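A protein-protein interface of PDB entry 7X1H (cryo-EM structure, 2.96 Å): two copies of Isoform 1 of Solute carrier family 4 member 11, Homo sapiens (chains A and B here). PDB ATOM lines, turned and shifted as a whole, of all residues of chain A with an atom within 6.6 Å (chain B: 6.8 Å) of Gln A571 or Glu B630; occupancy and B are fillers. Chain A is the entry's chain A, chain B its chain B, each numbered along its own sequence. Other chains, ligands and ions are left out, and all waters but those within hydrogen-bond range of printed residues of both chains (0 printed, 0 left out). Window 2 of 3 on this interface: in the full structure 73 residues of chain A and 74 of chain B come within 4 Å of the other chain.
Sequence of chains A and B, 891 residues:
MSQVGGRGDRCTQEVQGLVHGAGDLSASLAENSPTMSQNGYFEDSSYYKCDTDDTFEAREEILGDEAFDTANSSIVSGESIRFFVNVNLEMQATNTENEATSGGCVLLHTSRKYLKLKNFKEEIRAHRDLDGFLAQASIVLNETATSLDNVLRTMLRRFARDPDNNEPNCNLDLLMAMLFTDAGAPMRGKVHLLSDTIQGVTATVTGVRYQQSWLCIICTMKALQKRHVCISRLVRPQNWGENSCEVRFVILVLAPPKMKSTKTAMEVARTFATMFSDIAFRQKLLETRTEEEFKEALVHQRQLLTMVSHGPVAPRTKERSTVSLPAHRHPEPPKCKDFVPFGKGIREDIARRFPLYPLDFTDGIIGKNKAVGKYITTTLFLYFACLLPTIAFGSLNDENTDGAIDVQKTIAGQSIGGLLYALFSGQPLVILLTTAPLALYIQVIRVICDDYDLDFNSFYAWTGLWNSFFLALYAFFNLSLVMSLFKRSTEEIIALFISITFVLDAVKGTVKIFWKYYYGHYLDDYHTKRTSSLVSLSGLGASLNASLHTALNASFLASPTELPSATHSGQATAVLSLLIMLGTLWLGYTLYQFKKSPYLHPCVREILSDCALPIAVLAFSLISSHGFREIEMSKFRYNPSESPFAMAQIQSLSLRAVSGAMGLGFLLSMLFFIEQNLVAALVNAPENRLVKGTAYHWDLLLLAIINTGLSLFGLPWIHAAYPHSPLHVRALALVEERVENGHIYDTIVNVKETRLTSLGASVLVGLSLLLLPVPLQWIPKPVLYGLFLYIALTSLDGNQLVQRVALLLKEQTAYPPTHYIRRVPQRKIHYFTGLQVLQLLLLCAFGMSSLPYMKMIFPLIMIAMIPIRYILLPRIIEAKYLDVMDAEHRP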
ATOM      1  N   PHE A 514     -18.839   9.092  11.652  1.00  0.00           N
ATOM      2  CA  PHE A 514     -20.046   9.817  11.264  1.00  0.00           C
ATOM      3  C   PHE A 514     -21.298   9.010  11.580  1.00  0.00           C
ATOM      4  O   PHE A 514     -22.285   9.553  12.091  1.00  0.00           O
ATOM      5  CB  PHE A 514     -19.994  10.157   9.774  1.00  0.00           C
ATOM      6  CG  PHE A 514     -19.478  11.535   9.485  1.00  0.00           C
ATOM      7  CD1 PHE A 514     -18.138  11.838   9.659  1.00  0.00           C
ATOM      8  CD2 PHE A 514     -20.331  12.529   9.036  1.00  0.00           C
ATOM      9  CE1 PHE A 514     -17.661  13.106   9.393  1.00  0.00           C
ATOM     10  CE2 PHE A 514     -19.858  13.797   8.768  1.00  0.00           C
ATOM     11  CZ  PHE A 514     -18.521  14.086   8.947  1.00  0.00           C
ATOM     12  N   TYR A 517     -21.771   9.000  15.506  1.00  0.00           N
ATOM     13  CA  TYR A 517     -21.973  10.305  16.123  1.00  0.00           C
ATOM     14  C   TYR A 517     -22.893  11.211  15.313  1.00  0.00           C
ATOM     15  O   TYR A 517     -23.886  11.716  15.844  1.00  0.00           O
ATOM     16  CB  TYR A 517     -20.619  10.995  16.329  1.00  0.00           C
ATOM     17  CG  TYR A 517     -19.766  10.360  17.401  1.00  0.00           C
ATOM     18  CD1 TYR A 517     -20.038  10.566  18.747  1.00  0.00           C
ATOM     19  CD2 TYR A 517     -18.688   9.551  17.070  1.00  0.00           C
ATOM     20  CE1 TYR A 517     -19.261   9.988  19.730  1.00  0.00           C
ATOM     21  CE2 TYR A 517     -17.904   8.967  18.045  1.00  0.00           C
ATOM     22  CZ  TYR A 517     -18.195   9.189  19.373  1.00  0.00           C
ATOM     23  OH  TYR A 517     -17.418   8.611  20.350  1.00  0.00           O
ATOM     24  N   TYR A 518     -22.582  11.430  14.034  1.00  0.00           N
ATOM     25  CA  TYR A 518     -23.366  12.373  13.239  1.00  0.00           C
ATOM     26  C   TYR A 518     -24.817  11.927  13.123  1.00  0.00           C
ATOM     27  O   TYR A 518     -25.736  12.739  13.274  1.00  0.00           O
ATOM     28  CB  TYR A 518     -22.744  12.528  11.852  1.00  0.00           C
ATOM     29  CG  TYR A 518     -23.304  13.683  11.053  1.00  0.00           C
ATOM     30  CD1 TYR A 518     -22.734  14.945  11.130  1.00  0.00           C
ATOM     31  CD2 TYR A 518     -24.404  13.511  10.226  1.00  0.00           C
ATOM     32  CE1 TYR A 518     -23.242  16.003  10.404  1.00  0.00           C
ATOM     33  CE2 TYR A 518     -24.918  14.563   9.495  1.00  0.00           C
ATOM     34  CZ  TYR A 518     -24.334  15.806   9.588  1.00  0.00           C
ATOM     35  OH  TYR A 518     -24.841  16.858   8.863  1.00  0.00           O
ATOM     36  N   TYR A 519     -25.045  10.643  12.856  1.00  0.00           N
ATOM     37  CA  TYR A 519     -26.387  10.109  12.681  1.00  0.00           C
ATOM     38  C   TYR A 519     -26.963   9.515  13.959  1.00  0.00           C
ATOM     39  O   TYR A 519     -28.092   9.014  13.938  1.00  0.00           O
ATOM     40  CB  TYR A 519     -26.387   9.053  11.571  1.00  0.00           C
ATOM     41  CG  TYR A 519     -26.054   9.617  10.208  1.00  0.00           C
ATOM     42  CD1 TYR A 519     -26.888  10.543   9.597  1.00  0.00           C
ATOM     43  CD2 TYR A 519     -24.905   9.229   9.536  1.00  0.00           C
ATOM     44  CE1 TYR A 519     -26.589  11.064   8.354  1.00  0.00           C
ATOM     45  CE2 TYR A 519     -24.596   9.743   8.292  1.00  0.00           C
ATOM     46  CZ  TYR A 519     -25.441  10.660   7.705  1.00  0.00           C
ATOM     47  OH  TYR A 519     -25.139  11.177   6.467  1.00  0.00           O
ATOM     48  N   SER A 569     -24.817  15.965  20.644  1.00  0.00           N
ATOM     49  CA  SER A 569     -23.619  16.683  20.230  1.00  0.00           C
ATOM     50  C   SER A 569     -22.751  15.827  19.311  1.00  0.00           C
ATOM     51  O   SER A 569     -21.598  16.162  19.048  1.00  0.00           O
ATOM     52  CB  SER A 569     -22.812  17.123  21.454  1.00  0.00           C
ATOM     53  OG  SER A 569     -21.654  17.845  21.073  1.00  0.00           O
ATOM     54  N   GLY A 570     -23.314  14.720  18.822  1.00  0.00           N
ATOM     55  CA  GLY A 570     -22.556  13.836  17.955  1.00  0.00           C
ATOM     56  C   GLY A 570     -22.155  14.481  16.644  1.00  0.00           C
ATOM     57  O   GLY A 570     -21.074  14.204  16.118  1.00  0.00           O
ATOM     58  N   GLN A 571     -23.014  15.343  16.096  1.00  0.00           N
ATOM     59  CA  GLN A 571     -22.684  16.010  14.843  1.00  0.00           C
ATOM     60  C   GLN A 571     -21.424  16.852  14.991  1.00  0.00           C
ATOM     61  O   GLN A 571     -20.564  16.864  14.100  1.00  0.00           O
ATOM     62  CB  GLN A 571     -23.858  16.878  14.389  1.00  0.00           C
ATOM     63  CG  GLN A 571     -25.160  16.113  14.226  1.00  0.00           C
ATOM     64  CD  GLN A 571     -26.240  16.940  13.561  1.00  0.00           C
ATOM     65  OE1 GLN A 571     -26.241  18.167  13.649  1.00  0.00           O
ATOM     66  NE2 GLN A 571     -27.169  16.269  12.889  1.00  0.00           N
ATOM     67  N   ALA A 572     -21.298  17.564  16.112  1.00  0.00           N
ATOM     68  CA  ALA A 572     -20.095  18.353  16.351  1.00  0.00           C
ATOM     69  C   ALA A 572     -18.861  17.464  16.402  1.00  0.00           C
ATOM     70  O   ALA A 572     -17.822  17.798  15.821  1.00  0.00           O
ATOM     71  CB  ALA A 572     -20.239  19.147  17.649  1.00  0.00           C
ATOM     72  N   THR A 573     -18.957  16.320  17.086  1.00  0.00           N
ATOM     73  CA  THR A 573     -17.812  15.418  17.167  1.00  0.00           C
ATOM     74  C   THR A 573     -17.429  14.894  15.789  1.00  0.00           C
ATOM     75  O   THR A 573     -16.243  14.819  15.460  1.00  0.00           O
ATOM     76  CB  THR A 573     -18.110  14.251  18.109  1.00  0.00           C
ATOM     77  OG1 THR A 573     -19.083  13.386  17.513  1.00  0.00           O
ATOM     78  CG2 THR A 573     -18.620  14.746  19.454  1.00  0.00           C
ATOM     79  N   ALA A 574     -18.416  14.526  14.971  1.00  0.00           N
ATOM     80  CA  ALA A 574     -18.113  14.002  13.642  1.00  0.00           C
ATOM     81  C   ALA A 574     -17.460  15.063  12.764  1.00  0.00           C
ATOM     82  O   ALA A 574     -16.466  14.794  12.073  1.00  0.00           O
ATOM     83  CB  ALA A 574     -19.389  13.475  12.987  1.00  0.00           C
ATOM     84  N   VAL A 575     -18.006  16.283  12.774  1.00  0.00           N
ATOM     85  CA  VAL A 575     -17.443  17.345  11.947  1.00  0.00           C
ATOM     86  C   VAL A 575     -16.034  17.687  12.416  1.00  0.00           C
ATOM     87  O   VAL A 575     -15.128  17.905  11.602  1.00  0.00           O
ATOM     88  CB  VAL A 575     -18.363  18.579  11.953  1.00  0.00           C
ATOM     89  CG1 VAL A 575     -17.751  19.702  11.132  1.00  0.00           C
ATOM     90  CG2 VAL A 575     -19.737  18.222  11.407  1.00  0.00           C
ATOM     91  N   LEU A 576     -15.825  17.737  13.734  1.00  0.00           N
ATOM     92  CA  LEU A 576     -14.491  18.001  14.258  1.00  0.00           C
ATOM     93  C   LEU A 576     -13.528  16.880  13.899  1.00  0.00           C
ATOM     94  O   LEU A 576     -12.352  17.133  13.632  1.00  0.00           O
ATOM     95  CB  LEU A 576     -14.549  18.189  15.773  1.00  0.00           C
ATOM     96  CG  LEU A 576     -13.234  18.588  16.448  1.00  0.00           C
ATOM     97  CD1 LEU A 576     -12.606  19.794  15.768  1.00  0.00           C
ATOM     98  CD2 LEU A 576     -13.458  18.863  17.924  1.00  0.00           C
ATOM     99  N   SER B 569     -26.752  22.861  19.359  1.00  0.00           N
ATOM    100  CA  SER B 569     -26.021  22.386  18.190  1.00  0.00           C
ATOM    101  C   SER B 569     -25.100  23.470  17.638  1.00  0.00           C
ATOM    102  O   SER B 569     -24.584  23.348  16.529  1.00  0.00           O
ATOM    103  CB  SER B 569     -26.996  21.924  17.103  1.00  0.00           C
ATOM    104  OG  SER B 569     -26.304  21.435  15.967  1.00  0.00           O
ATOM    105  N   GLN B 571     -22.096  24.301  18.602  1.00  0.00           N
ATOM    106  CA  GLN B 571     -20.718  23.850  18.449  1.00  0.00           C
ATOM    107  C   GLN B 571     -20.505  23.197  17.091  1.00  0.00           C
ATOM    108  O   GLN B 571     -19.480  23.424  16.435  1.00  0.00           O
ATOM    109  CB  GLN B 571     -20.361  22.880  19.574  1.00  0.00           C
ATOM    110  CG  GLN B 571     -20.555  23.453  20.967  1.00  0.00           C
ATOM    111  CD  GLN B 571     -19.981  22.563  22.049  1.00  0.00           C
ATOM    112  OE1 GLN B 571     -19.882  21.347  21.881  1.00  0.00           O
ATOM    113  NE2 GLN B 571     -19.600  23.164  23.171  1.00  0.00           N
ATOM    114  N   ALA B 572     -21.464  22.378  16.655  1.00  0.00           N
ATOM    115  CA  ALA B 572     -21.358  21.757  15.341  1.00  0.00           C
ATOM    116  C   ALA B 572     -21.316  22.809  14.243  1.00  0.00           C
ATOM    117  O   ALA B 572     -20.513  22.709  13.309  1.00  0.00           O
ATOM    118  CB  ALA B 572     -22.526  20.797  15.120  1.00  0.00           C
ATOM    119  N   VAL B 575     -17.813  24.545  14.290  1.00  0.00           N
ATOM    120  CA  VAL B 575     -16.746  23.689  13.778  1.00  0.00           C
ATOM    121  C   VAL B 575     -16.893  23.508  12.273  1.00  0.00           C
ATOM    122  O   VAL B 575     -15.904  23.528  11.530  1.00  0.00           O
ATOM    123  CB  VAL B 575     -16.736  22.338  14.519  1.00  0.00           C
ATOM    124  CG1 VAL B 575     -15.658  21.431  13.951  1.00  0.00           C
ATOM    125  CG2 VAL B 575     -16.510  22.549  16.008  1.00  0.00           C
ATOM    126  N   SER B 624     -21.628  22.354   2.171  1.00  0.00           N
ATOM    127  CA  SER B 624     -22.173  22.907   3.404  1.00  0.00           C
ATOM    128  C   SER B 624     -23.685  23.082   3.373  1.00  0.00           C
ATOM    129  O   SER B 624     -24.288  23.266   4.436  1.00  0.00           O
ATOM    130  CB  SER B 624     -21.516  24.256   3.697  1.00  0.00           C
ATOM    131  OG  SER B 624     -22.298  25.014   4.601  1.00  0.00           O
ATOM    132  N   SER B 625     -24.313  23.031   2.197  1.00  0.00           N
ATOM    133  CA  SER B 625     -25.756  23.184   2.089  1.00  0.00           C
ATOM    134  C   SER B 625     -26.480  21.895   1.734  1.00  0.00           C
ATOM    135  O   SER B 625     -27.682  21.793   1.990  1.00  0.00           O
ATOM    136  CB  SER B 625     -26.101  24.248   1.035  1.00  0.00           C
ATOM    137  OG  SER B 625     -25.572  25.512   1.398  1.00  0.00           O
ATOM    138  N   HIS B 626     -25.784  20.917   1.156  1.00  0.00           N
ATOM    139  CA  HIS B 626     -26.377  19.633   0.808  1.00  0.00           C
ATOM    140  C   HIS B 626     -25.740  18.481   1.566  1.00  0.00           C
ATOM    141  O   HIS B 626     -26.456  17.641   2.124  1.00  0.00           O
ATOM    142  CB  HIS B 626     -26.255  19.393  -0.706  1.00  0.00           C
ATOM    143  CG  HIS B 626     -27.346  18.539  -1.271  1.00  0.00           C
ATOM    144  ND1 HIS B 626     -27.326  17.162  -1.204  1.00  0.00           N
ATOM    145  CD2 HIS B 626     -28.493  18.867  -1.911  1.00  0.00           C
ATOM    146  CE1 HIS B 626     -28.411  16.679  -1.780  1.00  0.00           C
ATOM    147  NE2 HIS B 626     -29.137  17.693  -2.217  1.00  0.00           N
ATOM    148  N   GLY B 627     -24.408  18.417   1.608  1.00  0.00           N
ATOM    149  CA  GLY B 627     -23.755  17.366   2.368  1.00  0.00           C
ATOM    150  C   GLY B 627     -23.983  17.500   3.861  1.00  0.00           C
ATOM    151  O   GLY B 627     -24.152  16.499   4.564  1.00  0.00           O
ATOM    152  N   PHE B 628     -23.991  18.730   4.366  1.00  0.00           N
ATOM    153  CA  PHE B 628     -24.188  19.020   5.780  1.00  0.00           C
ATOM    154  C   PHE B 628     -25.462  19.830   5.992  1.00  0.00           C
ATOM    155  O   PHE B 628     -25.504  20.762   6.796  1.00  0.00           O
ATOM    156  CB  PHE B 628     -22.983  19.764   6.353  1.00  0.00           C
ATOM    157  CG  PHE B 628     -21.777  18.895   6.568  1.00  0.00           C
ATOM    158  CD1 PHE B 628     -21.776  17.920   7.549  1.00  0.00           C
ATOM    159  CD2 PHE B 628     -20.644  19.057   5.790  1.00  0.00           C
ATOM    160  CE1 PHE B 628     -20.666  17.122   7.751  1.00  0.00           C
ATOM    161  CE2 PHE B 628     -19.533  18.263   5.986  1.00  0.00           C
ATOM    162  CZ  PHE B 628     -19.544  17.293   6.968  1.00  0.00           C
ATOM    163  N   ARG B 629     -26.526  19.476   5.266  1.00  0.00           N
ATOM    164  CA  ARG B 629     -27.776  20.221   5.372  1.00  0.00           C
ATOM    165  C   ARG B 629     -28.397  20.122   6.758  1.00  0.00           C
ATOM    166  O   ARG B 629     -29.173  21.005   7.138  1.00  0.00           O
ATOM    167  CB  ARG B 629     -28.770  19.727   4.320  1.00  0.00           C
ATOM    168  CG  ARG B 629     -29.246  18.298   4.527  1.00  0.00           C
ATOM    169  CD  ARG B 629     -30.133  17.842   3.382  1.00  0.00           C
ATOM    170  NE  ARG B 629     -30.665  16.502   3.599  1.00  0.00           N
ATOM    171  CZ  ARG B 629     -30.046  15.379   3.259  1.00  0.00           C
ATOM    172  NH1 ARG B 629     -28.854  15.392   2.683  1.00  0.00           N
ATOM    173  NH2 ARG B 629     -30.637  14.213   3.503  1.00  0.00           N
ATOM    174  N   GLU B 630     -28.074  19.076   7.522  1.00  0.00           N
ATOM    175  CA  GLU B 630     -28.608  18.950   8.872  1.00  0.00           C
ATOM    176  C   GLU B 630     -28.034  19.995   9.818  1.00  0.00           C
ATOM    177  O   GLU B 630     -28.613  20.232  10.883  1.00  0.00           O
ATOM    178  CB  GLU B 630     -28.330  17.549   9.419  1.00  0.00           C
ATOM    179  CG  GLU B 630     -28.926  16.428   8.584  1.00  0.00           C
ATOM    180  CD  GLU B 630     -27.868  15.582   7.903  1.00  0.00           C
ATOM    181  OE1 GLU B 630     -26.997  16.156   7.216  1.00  0.00           O
ATOM    182  OE2 GLU B 630     -27.908  14.344   8.055  1.00  0.00           O
ATOM    183  N   ILE B 631     -26.915  20.622   9.457  1.00  0.00           N
ATOM    184  CA  ILE B 631     -26.288  21.637  10.297  1.00  0.00           C
ATOM    185  C   ILE B 631     -26.506  23.008   9.674  1.00  0.00           C
ATOM    186  O   ILE B 631     -25.720  23.450   8.828  1.00  0.00           O
ATOM    187  CB  ILE B 631     -24.785  21.351  10.487  1.00  0.00           C
ATOM    188  CG1 ILE B 631     -24.577  19.908  10.956  1.00  0.00           C
ATOM    189  CG2 ILE B 631     -24.178  22.337  11.478  1.00  0.00           C
ATOM    190  CD1 ILE B 631     -23.139  19.560  11.277  1.00  0.00           C
ATOM    191  N   GLU B 632     -27.570  23.690  10.086  1.00  0.00           N
ATOM    192  CA  GLU B 632     -27.816  25.043   9.614  1.00  0.00           C
ATOM    193  C   GLU B 632     -26.779  25.996  10.194  1.00  0.00           C
ATOM    194  O   GLU B 632     -26.378  25.870  11.355  1.00  0.00           O
ATOM    195  CB  GLU B 632     -29.224  25.496  10.001  1.00  0.00           C
ATOM    196  CG  GLU B 632     -29.472  25.556  11.504  1.00  0.00           C
ATOM    197  CD  GLU B 632     -29.172  26.920  12.103  1.00  0.00           C
ATOM    198  OE1 GLU B 632     -29.195  27.923  11.360  1.00  0.00           O
ATOM    199  OE2 GLU B 632     -28.911  26.987  13.322  1.00  0.00           O
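The side-chain carboxylate (OE1) of Glu B630 lies within hydrogen-bond range of the side-chain hydroxyl (OH) of Tyr A518, at 2.8 Å.
The backbone carbonyl oxygen of Phe A514 lies within hydrogen-bond range of the backbone NH of Tyr A519 (3.1 Å).
Phe B628 touches Phe A514. Phe B628 touches Tyr A518 (CD1 to OH, 3.5 Å). CD1 of Ile B631 touches CE1 of Tyr A518, 3.7 Å away. Tyr A519 touches Glu B630 (CE1 to OE2, 3.5 Å). Glu B630 touches Gln A571. OE1 of Gln A571 touches CG1 of Ile B631 (3.6 Å). CB of Ala A572 touches N of Ala B572, 3.6 Å away. Val B575 touches Val A575. Val A575 touches Phe B628. Leu A576 touches Val B575 (CA to CG1, 3.6 Å).
Of the printed residues of chain B, Gln A571 touches Glu B630 (3.9 Å) and Ile B631 (3.6 Å). Of chain A, only Tyr A518, Tyr A519 and Gln A571 come within 4 Å of Glu B630. Of the printed residues of chain A, Ile B631 touches Tyr A518, Gln A571 and Val A575. Printed residues of chain B within 4 Å of Tyr A519: Glu B630. Of the printed residues of chain B, Ala A572 touches Ala B572. Ser B569 touches none of the printed residues of chain A. The nearest printed residue of chain A that does not touch Glu B630 is Phe A514 (7.7 Å).
Printed residues of chain A that touch a printed residue of chain B: Phe A514, Tyr A518, Tyr A519, Gln A571, Ala A572, Val A575 and Leu A576. Hydrophobic or aromatic side chains of chain A that line the printed part of chain B: Phe A514, Tyr A518, Tyr A519, Ala A572, Val A575 and Leu A576.
Ala B572 touches its own counterpart, Ala A572. Val A575 touches its own counterpart, Val B575. Positions printed for both chains: 569, 571, 572 and 575.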
